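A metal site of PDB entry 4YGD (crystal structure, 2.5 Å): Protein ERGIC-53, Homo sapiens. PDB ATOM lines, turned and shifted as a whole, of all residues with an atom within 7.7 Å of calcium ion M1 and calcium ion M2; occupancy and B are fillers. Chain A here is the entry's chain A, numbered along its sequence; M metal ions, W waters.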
ATOM      1  N   GLY A  96     -16.857  -6.995  20.121  1.00  0.00           N
ATOM      2  CA  GLY A  96     -15.417  -7.086  20.341  1.00  0.00           C
ATOM      3  C   GLY A  96     -15.040  -8.178  21.341  1.00  0.00           C
ATOM      4  O   GLY A  96     -15.899  -8.802  21.921  1.00  0.00           O
ATOM      5  N   ALA A  97     -13.751  -8.401  21.531  1.00  0.00           N
ATOM      6  CA  ALA A  97     -13.306  -9.401  22.493  1.00  0.00           C
ATOM      7  C   ALA A  97     -11.831  -9.205  22.819  1.00  0.00           C
ATOM      8  O   ALA A  97     -11.144  -8.551  22.050  1.00  0.00           O
ATOM      9  CB  ALA A  97     -13.521 -10.812  21.933  1.00  0.00           C
ATOM     10  N   ASP A  98     -11.353  -9.730  23.930  1.00  0.00           N
ATOM     11  CA  ASP A  98     -12.156 -10.390  24.964  1.00  0.00           C
ATOM     12  C   ASP A  98     -12.511  -9.475  26.105  1.00  0.00           C
ATOM     13  O   ASP A  98     -13.558  -9.633  26.726  1.00  0.00           O
ATOM     14  CB  ASP A  98     -11.414 -11.591  25.550  1.00  0.00           C
ATOM     15  CG  ASP A  98     -11.690 -12.872  24.790  1.00  0.00           C
ATOM     16  OD1 ASP A  98     -10.733 -13.407  24.238  1.00  0.00           O
ATOM     17  OD2 ASP A  98     -12.865 -13.321  24.743  1.00  0.00           O
ATOM     18  N   GLY A  99     -11.598  -8.548  26.400  1.00  0.00           N
ATOM     19  CA  GLY A  99     -11.815  -7.603  27.434  1.00  0.00           C
ATOM     20  C   GLY A  99     -10.587  -7.467  28.285  1.00  0.00           C
ATOM     21  O   GLY A  99      -9.523  -7.980  27.958  1.00  0.00           O
ATOM     22  N   PHE A 115      -8.347 -13.435  30.958  1.00  0.00           N
ATOM     23  CA  PHE A 115      -8.039 -12.160  30.351  1.00  0.00           C
ATOM     24  C   PHE A 115      -6.528 -11.886  30.347  1.00  0.00           C
ATOM     25  O   PHE A 115      -6.063 -10.826  30.735  1.00  0.00           O
ATOM     26  CB  PHE A 115      -8.812 -11.091  31.069  1.00  0.00           C
ATOM     27  CG  PHE A 115     -10.283 -11.237  30.922  1.00  0.00           C
ATOM     28  CD1 PHE A 115     -10.911 -10.733  29.825  1.00  0.00           C
ATOM     29  CD2 PHE A 115     -11.036 -11.875  31.878  1.00  0.00           C
ATOM     30  CE1 PHE A 115     -12.283 -10.846  29.692  1.00  0.00           C
ATOM     31  CE2 PHE A 115     -12.409 -11.996  31.738  1.00  0.00           C
ATOM     32  CZ  PHE A 115     -13.035 -11.484  30.648  1.00  0.00           C
ATOM     33  N   PHE A 128     -13.836  -6.629  32.754  1.00  0.00           N
ATOM     34  CA  PHE A 128     -14.545  -5.867  31.737  1.00  0.00           C
ATOM     35  C   PHE A 128     -14.620  -6.761  30.510  1.00  0.00           C
ATOM     36  O   PHE A 128     -13.718  -6.824  29.687  1.00  0.00           O
ATOM     37  CB  PHE A 128     -13.794  -4.578  31.451  1.00  0.00           C
ATOM     38  CG  PHE A 128     -13.675  -3.684  32.653  1.00  0.00           C
ATOM     39  CD1 PHE A 128     -14.507  -2.581  32.777  1.00  0.00           C
ATOM     40  CD2 PHE A 128     -12.807  -3.973  33.661  1.00  0.00           C
ATOM     41  CE1 PHE A 128     -14.414  -1.776  33.902  1.00  0.00           C
ATOM     42  CE2 PHE A 128     -12.695  -3.163  34.775  1.00  0.00           C
ATOM     43  CZ  PHE A 128     -13.497  -2.069  34.901  1.00  0.00           C
ATOM     44  N   ASP A 129     -15.737  -7.455  30.405  1.00  0.00           N
ATOM     45  CA  ASP A 129     -15.883  -8.586  29.520  1.00  0.00           C
ATOM     46  C   ASP A 129     -16.707  -8.145  28.321  1.00  0.00           C
ATOM     47  O   ASP A 129     -17.911  -7.914  28.432  1.00  0.00           O
ATOM     48  CB  ASP A 129     -16.602  -9.696  30.307  1.00  0.00           C
ATOM     49  CG  ASP A 129     -16.642 -10.999  29.596  1.00  0.00           C
ATOM     50  OD1 ASP A 129     -16.595 -11.033  28.354  1.00  0.00           O
ATOM     51  OD2 ASP A 129     -16.738 -12.031  30.280  1.00  0.00           O
ATOM     52  N   SER A 130     -16.043  -7.999  27.204  1.00  0.00           N
ATOM     53  CA  SER A 130     -16.667  -7.533  25.958  1.00  0.00           C
ATOM     54  C   SER A 130     -17.507  -8.639  25.278  1.00  0.00           C
ATOM     55  O   SER A 130     -18.457  -8.335  24.578  1.00  0.00           O
ATOM     56  CB  SER A 130     -15.576  -7.194  24.944  1.00  0.00           C
ATOM     57  OG  SER A 130     -14.893  -6.047  25.335  1.00  0.00           O
ATOM     58  N   PHE A 131     -17.090  -9.902  25.433  1.00  0.00           N
ATOM     59  CA  PHE A 131     -17.604 -10.929  24.564  1.00  0.00           C
ATOM     60  C   PHE A 131     -18.523 -11.890  25.310  1.00  0.00           C
ATOM     61  O   PHE A 131     -18.125 -12.537  26.304  1.00  0.00           O
ATOM     62  CB  PHE A 131     -16.478 -11.679  23.855  1.00  0.00           C
ATOM     63  CG  PHE A 131     -16.968 -12.633  22.791  1.00  0.00           C
ATOM     64  CD1 PHE A 131     -17.411 -12.156  21.563  1.00  0.00           C
ATOM     65  CD2 PHE A 131     -17.022 -14.011  23.036  1.00  0.00           C
ATOM     66  CE1 PHE A 131     -17.887 -13.039  20.582  1.00  0.00           C
ATOM     67  CE2 PHE A 131     -17.510 -14.887  22.066  1.00  0.00           C
ATOM     68  CZ  PHE A 131     -17.947 -14.399  20.838  1.00  0.00           C
ATOM     69  N   ASP A 132     -19.730 -11.989  24.747  1.00  0.00           N
ATOM     70  CA  ASP A 132     -20.854 -12.776  25.256  1.00  0.00           C
ATOM     71  C   ASP A 132     -20.679 -14.272  24.971  1.00  0.00           C
ATOM     72  O   ASP A 132     -21.261 -14.809  24.045  1.00  0.00           O
ATOM     73  CB  ASP A 132     -22.138 -12.257  24.597  1.00  0.00           C
ATOM     74  CG  ASP A 132     -23.396 -12.727  25.267  1.00  0.00           C
ATOM     75  OD1 ASP A 132     -23.367 -13.168  26.463  1.00  0.00           O
ATOM     76  OD2 ASP A 132     -24.434 -12.610  24.574  1.00  0.00           O
ATOM     77  N   ASN A 133     -19.890 -14.936  25.813  1.00  0.00           N
ATOM     78  CA  ASN A 133     -19.499 -16.320  25.579  1.00  0.00           C
ATOM     79  C   ASN A 133     -20.685 -17.298  25.690  1.00  0.00           C
ATOM     80  O   ASN A 133     -20.773 -18.229  24.906  1.00  0.00           O
ATOM     81  CB  ASN A 133     -18.396 -16.712  26.572  1.00  0.00           C
ATOM     82  CG  ASN A 133     -17.026 -16.198  26.147  1.00  0.00           C
ATOM     83  OD1 ASN A 133     -16.577 -15.129  26.560  1.00  0.00           O
ATOM     84  ND2 ASN A 133     -16.362 -16.964  25.312  1.00  0.00           N
ATOM     85  N   ASP A 134     -21.574 -17.050  26.655  1.00  0.00           N
ATOM     86  CA  ASP A 134     -22.765 -17.873  26.871  1.00  0.00           C
ATOM     87  C   ASP A 134     -23.999 -17.356  26.129  1.00  0.00           C
ATOM     88  O   ASP A 134     -25.128 -17.696  26.493  1.00  0.00           O
ATOM     89  CB  ASP A 134     -23.089 -17.940  28.370  1.00  0.00           C
ATOM     90  CG  ASP A 134     -23.266 -16.543  29.027  1.00  0.00           C
ATOM     91  OD1 ASP A 134     -23.264 -15.513  28.296  1.00  0.00           O
ATOM     92  OD2 ASP A 134     -23.412 -16.477  30.262  1.00  0.00           O
ATOM     93  N   GLY A 135     -23.810 -16.491  25.129  1.00  0.00           N
ATOM     94  CA  GLY A 135     -24.922 -16.025  24.294  1.00  0.00           C
ATOM     95  C   GLY A 135     -26.147 -15.413  24.949  1.00  0.00           C
ATOM     96  O   GLY A 135     -27.200 -15.370  24.321  1.00  0.00           O
ATOM     97  N   LYS A 136     -26.006 -14.899  26.182  1.00  0.00           N
ATOM     98  CA  LYS A 136     -27.124 -14.278  26.930  1.00  0.00           C
ATOM     99  C   LYS A 136     -27.426 -12.775  26.636  1.00  0.00           C
ATOM    100  O   LYS A 136     -28.172 -12.147  27.401  1.00  0.00           O
ATOM    101  CB  LYS A 136     -26.910 -14.443  28.450  1.00  0.00           C
ATOM    102  CG  LYS A 136     -26.829 -15.873  28.958  1.00  0.00           C
ATOM    103  CD  LYS A 136     -28.162 -16.606  28.889  1.00  0.00           C
ATOM    104  CE  LYS A 136     -28.012 -18.111  29.166  1.00  0.00           C
ATOM    105  NZ  LYS A 136     -29.093 -18.934  28.549  1.00  0.00           N
ATOM    106  N   LYS A 137     -26.876 -12.229  25.550  1.00  0.00           N
ATOM    107  CA  LYS A 137     -27.097 -10.834  25.113  1.00  0.00           C
ATOM    108  C   LYS A 137     -27.016  -9.818  26.246  1.00  0.00           C
ATOM    109  O   LYS A 137     -27.756  -8.849  26.292  1.00  0.00           O
ATOM    110  CB  LYS A 137     -28.415 -10.700  24.316  1.00  0.00           C
ATOM    111  CG  LYS A 137     -28.546 -11.753  23.233  1.00  0.00           C
ATOM    112  CD  LYS A 137     -29.417 -11.393  22.069  1.00  0.00           C
ATOM    113  CE  LYS A 137     -29.412 -12.678  21.257  1.00  0.00           C
ATOM    114  NZ  LYS A 137     -30.211 -12.626  20.025  1.00  0.00           N
ATOM    115  N   ASN A 138     -26.070 -10.053  27.149  1.00  0.00           N
ATOM    116  CA  ASN A 138     -25.861  -9.176  28.303  1.00  0.00           C
ATOM    117  C   ASN A 138     -24.383  -8.690  28.411  1.00  0.00           C
ATOM    118  O   ASN A 138     -23.783  -8.714  29.492  1.00  0.00           O
ATOM    119  CB  ASN A 138     -26.290  -9.935  29.558  1.00  0.00           C
ATOM    120  CG  ASN A 138     -25.558 -11.240  29.706  1.00  0.00           C
ATOM    121  OD1 ASN A 138     -24.946 -11.736  28.742  1.00  0.00           O
ATOM    122  ND2 ASN A 138     -25.538 -11.774  30.911  1.00  0.00           N
ATOM    123  N   ASN A 139     -23.807  -8.272  27.274  1.00  0.00           N
ATOM    124  CA  ASN A 139     -22.431  -7.772  27.205  1.00  0.00           C
ATOM    125  C   ASN A 139     -22.400  -6.534  26.317  1.00  0.00           C
ATOM    126  O   ASN A 139     -23.212  -6.410  25.432  1.00  0.00           O
ATOM    127  CB  ASN A 139     -21.458  -8.812  26.625  1.00  0.00           C
ATOM    128  CG  ASN A 139     -21.330 -10.052  27.504  1.00  0.00           C
ATOM    129  OD1 ASN A 139     -22.226 -10.900  27.513  1.00  0.00           O
ATOM    130  ND2 ASN A 139     -20.201 -10.190  28.208  1.00  0.00           N
ATOM    131  N   PRO A 140     -21.431  -5.644  26.520  1.00  0.00           N
ATOM    132  CA  PRO A 140     -20.358  -5.724  27.497  1.00  0.00           C
ATOM    133  C   PRO A 140     -20.834  -5.670  28.941  1.00  0.00           C
ATOM    134  O   PRO A 140     -21.836  -5.046  29.241  1.00  0.00           O
ATOM    135  CB  PRO A 140     -19.514  -4.511  27.164  1.00  0.00           C
ATOM    136  CG  PRO A 140     -19.715  -4.315  25.695  1.00  0.00           C
ATOM    137  CD  PRO A 140     -21.178  -4.595  25.507  1.00  0.00           C
ATOM    138  N   ALA A 141     -20.124  -6.371  29.810  1.00  0.00           N
ATOM    139  CA  ALA A 141     -20.431  -6.420  31.216  1.00  0.00           C
ATOM    140  C   ALA A 141     -19.190  -6.217  32.040  1.00  0.00           C
ATOM    141  O   ALA A 141     -18.094  -6.451  31.598  1.00  0.00           O
ATOM    142  CB  ALA A 141     -21.082  -7.777  31.588  1.00  0.00           C
ATOM    143  N   TYR A 153     -11.743 -20.002  36.672  1.00  0.00           N
ATOM    144  CA  TYR A 153     -12.633 -19.048  36.026  1.00  0.00           C
ATOM    145  C   TYR A 153     -13.464 -19.682  34.884  1.00  0.00           C
ATOM    146  O   TYR A 153     -12.941 -20.308  33.958  1.00  0.00           O
ATOM    147  CB  TYR A 153     -11.869 -17.801  35.520  1.00  0.00           C
ATOM    148  CG  TYR A 153     -12.716 -16.907  34.606  1.00  0.00           C
ATOM    149  CD1 TYR A 153     -13.747 -16.116  35.106  1.00  0.00           C
ATOM    150  CD2 TYR A 153     -12.477 -16.868  33.242  1.00  0.00           C
ATOM    151  CE1 TYR A 153     -14.506 -15.322  34.256  1.00  0.00           C
ATOM    152  CE2 TYR A 153     -13.231 -16.093  32.381  1.00  0.00           C
ATOM    153  CZ  TYR A 153     -14.242 -15.330  32.876  1.00  0.00           C
ATOM    154  OH  TYR A 153     -14.982 -14.555  32.011  1.00  0.00           O
ATOM    155  N   ASP A 154     -14.763 -19.435  34.947  1.00  0.00           N
ATOM    156  CA  ASP A 154     -15.718 -19.962  34.003  1.00  0.00           C
ATOM    157  C   ASP A 154     -15.861 -19.055  32.771  1.00  0.00           C
ATOM    158  O   ASP A 154     -16.791 -18.249  32.669  1.00  0.00           O
ATOM    159  CB  ASP A 154     -17.074 -20.133  34.728  1.00  0.00           C
ATOM    160  CG  ASP A 154     -18.060 -20.989  33.949  1.00  0.00           C
ATOM    161  OD1 ASP A 154     -17.676 -21.581  32.923  1.00  0.00           O
ATOM    162  OD2 ASP A 154     -19.250 -21.009  34.338  1.00  0.00           O
ATOM    163  N   HIS A 155     -14.904 -19.180  31.852  1.00  0.00           N
ATOM    164  CA  HIS A 155     -14.893 -18.474  30.568  1.00  0.00           C
ATOM    165  C   HIS A 155     -16.187 -18.541  29.779  1.00  0.00           C
ATOM    166  O   HIS A 155     -16.656 -17.540  29.253  1.00  0.00           O
ATOM    167  CB  HIS A 155     -13.853 -19.120  29.647  1.00  0.00           C
ATOM    168  CG  HIS A 155     -12.451 -19.042  30.168  1.00  0.00           C
ATOM    169  ND1 HIS A 155     -11.660 -17.926  30.002  1.00  0.00           N
ATOM    170  CD2 HIS A 155     -11.698 -19.957  30.825  1.00  0.00           C
ATOM    171  CE1 HIS A 155     -10.470 -18.159  30.542  1.00  0.00           C
ATOM    172  NE2 HIS A 155     -10.471 -19.379  31.046  1.00  0.00           N
ATOM    173  N   GLN A 156     -16.735 -19.740  29.651  1.00  0.00           N
ATOM    174  CA  GLN A 156     -17.882 -19.962  28.766  1.00  0.00           C
ATOM    175  C   GLN A 156     -19.120 -19.231  29.204  1.00  0.00           C
ATOM    176  O   GLN A 156     -19.940 -18.859  28.376  1.00  0.00           O
ATOM    177  CB  GLN A 156     -18.170 -21.458  28.639  1.00  0.00           C
ATOM    178  CG  GLN A 156     -17.041 -22.183  27.892  1.00  0.00           C
ATOM    179  CD  GLN A 156     -16.121 -22.990  28.815  1.00  0.00           C
ATOM    180  OE1 GLN A 156     -15.910 -22.654  29.992  1.00  0.00           O
ATOM    181  NE2 GLN A 156     -15.550 -24.061  28.265  1.00  0.00           N
ATOM    182  N   ASN A 157     -19.257 -19.024  30.512  1.00  0.00           N
ATOM    183  CA  ASN A 157     -20.424 -18.329  31.069  1.00  0.00           C
ATOM    184  C   ASN A 157     -20.137 -16.916  31.522  1.00  0.00           C
ATOM    185  O   ASN A 157     -20.918 -16.334  32.313  1.00  0.00           O
ATOM    186  CB  ASN A 157     -21.030 -19.146  32.211  1.00  0.00           C
ATOM    187  CG  ASN A 157     -21.500 -20.511  31.741  1.00  0.00           C
ATOM    188  OD1 ASN A 157     -22.551 -20.632  31.104  1.00  0.00           O
ATOM    189  ND2 ASN A 157     -20.717 -21.547  32.023  1.00  0.00           N
ATOM    190  N   ASP A 158     -19.033 -16.329  31.048  1.00  0.00           N
ATOM    191  CA  ASP A 158     -18.689 -14.956  31.440  1.00  0.00           C
ATOM    192  C   ASP A 158     -18.639 -14.805  32.959  1.00  0.00           C
ATOM    193  O   ASP A 158     -19.077 -13.794  33.507  1.00  0.00           O
ATOM    194  CB  ASP A 158     -19.704 -13.957  30.851  1.00  0.00           C
ATOM    195  CG  ASP A 158     -19.715 -13.967  29.354  1.00  0.00           C
ATOM    196  OD1 ASP A 158     -18.644 -14.273  28.790  1.00  0.00           O
ATOM    197  OD2 ASP A 158     -20.761 -13.635  28.737  1.00  0.00           O
ATOM    198  N   GLY A 159     -18.171 -15.843  33.637  1.00  0.00           N
ATOM    199  CA  GLY A 159     -18.216 -15.923  35.108  1.00  0.00           C
ATOM    200  C   GLY A 159     -19.555 -15.735  35.800  1.00  0.00           C
ATOM    201  O   GLY A 159     -19.584 -15.442  37.008  1.00  0.00           O
ATOM    202  N   ALA A 160     -20.666 -15.935  35.098  1.00  0.00           N
ATOM    203  CA  ALA A 160     -22.015 -15.623  35.640  1.00  0.00           C
ATOM    204  C   ALA A 160     -22.352 -16.282  36.973  1.00  0.00           C
ATOM    205  O   ALA A 160     -23.000 -15.664  37.824  1.00  0.00           O
ATOM    206  CB  ALA A 160     -23.115 -15.942  34.625  1.00  0.00           C
ATOM    207  N   GLN A 168     -24.162  -4.074  33.634  1.00  0.00           N
ATOM    208  CA  GLN A 168     -24.029  -4.013  32.189  1.00  0.00           C
ATOM    209  C   GLN A 168     -23.640  -2.604  31.830  1.00  0.00           C
ATOM    210  O   GLN A 168     -24.184  -1.686  32.354  1.00  0.00           O
ATOM    211  CB  GLN A 168     -25.319  -4.413  31.531  1.00  0.00           C
ATOM    212  CG  GLN A 168     -25.596  -5.890  31.729  1.00  0.00           C
ATOM    213  CD  GLN A 168     -26.410  -6.420  30.609  1.00  0.00           C
ATOM    214  OE1 GLN A 168     -27.441  -7.057  30.814  1.00  0.00           O
ATOM    215  NE2 GLN A 168     -25.989  -6.114  29.379  1.00  0.00           N
HETATM  216 CA    CA M   1     -16.697 -13.328  27.933  1.00  0.00          CA
HETATM  217 CA    CA M   2     -22.853 -12.946  28.698  1.00  0.00          CA
HETATM  218  O   HOH W   1     -14.752 -12.666  26.699  1.00  0.00           O
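Within 4 Å of calcium ion M1: Asp 129, Phe 131, Asn 133 and Asp 158.
The nearest printed residue that does not touch calcium ion M1 is His 155 (4.4 Å).
Calcium ion M2 is bound by the side-chain carboxylate (OD2) of Asp 158 (2.2 Å), the side-chain carboxylate (OD1) of Asp 132 (2.3 Å), the side-chain amide oxygen (OD1) of Asn 138 (2.4 Å), the side-chain amide oxygen (OD1) of Asn 139 (2.4 Å) and the side-chain carboxylate (OD1) of Asp 134 (2.6 Å).
Calcium ion M2 has five donor atoms within binding distance.
The backbone NH (N) of Lys 136 lies within hydrogen-bond range of the side-chain carboxylate (OD2) of Asp 132 (3.2 Å).
The backbone NH of Lys 137 lies within hydrogen-bond range of the side-chain carboxylate of Asp 132, 2.7 Å away.
The backbone carbonyl oxygen of Asp 129 is in hydrogen-bond range of the side-chain amide nitrogen of Asn 139 (3.2 Å).
The backbone NH (N) of Asp 129 sits at hydrogen-bond distance from the backbone carbonyl oxygen (O) of Ala 141.
The backbone carbonyl oxygen of Asn 138 lies close to the side-chain amide nitrogen of Gln 168 (3.4 Å).
N of Asp 134 lies within hydrogen-bond range of O of Gln 156.
OD1 of Asn 133 binds calcium ion M1.
O of Phe 131 binds calcium ion M1 (2.3 Å).
OD1 of Asp 158 binds calcium ion M1 (2.3 Å).
Calcium ion M1 is bound by OD1 of Asp 129 (2.3 Å).
Water W1 binds calcium ion M1 (2.4 Å).
OD2 of Asp 129 binds calcium ion M1, 2.7 Å away.
Of the 28 residues printed, 5 come within 4 Å of calcium ion M2.
The nearest printed residue that does not touch calcium ion M2 is Lys 136 (4.3 Å).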
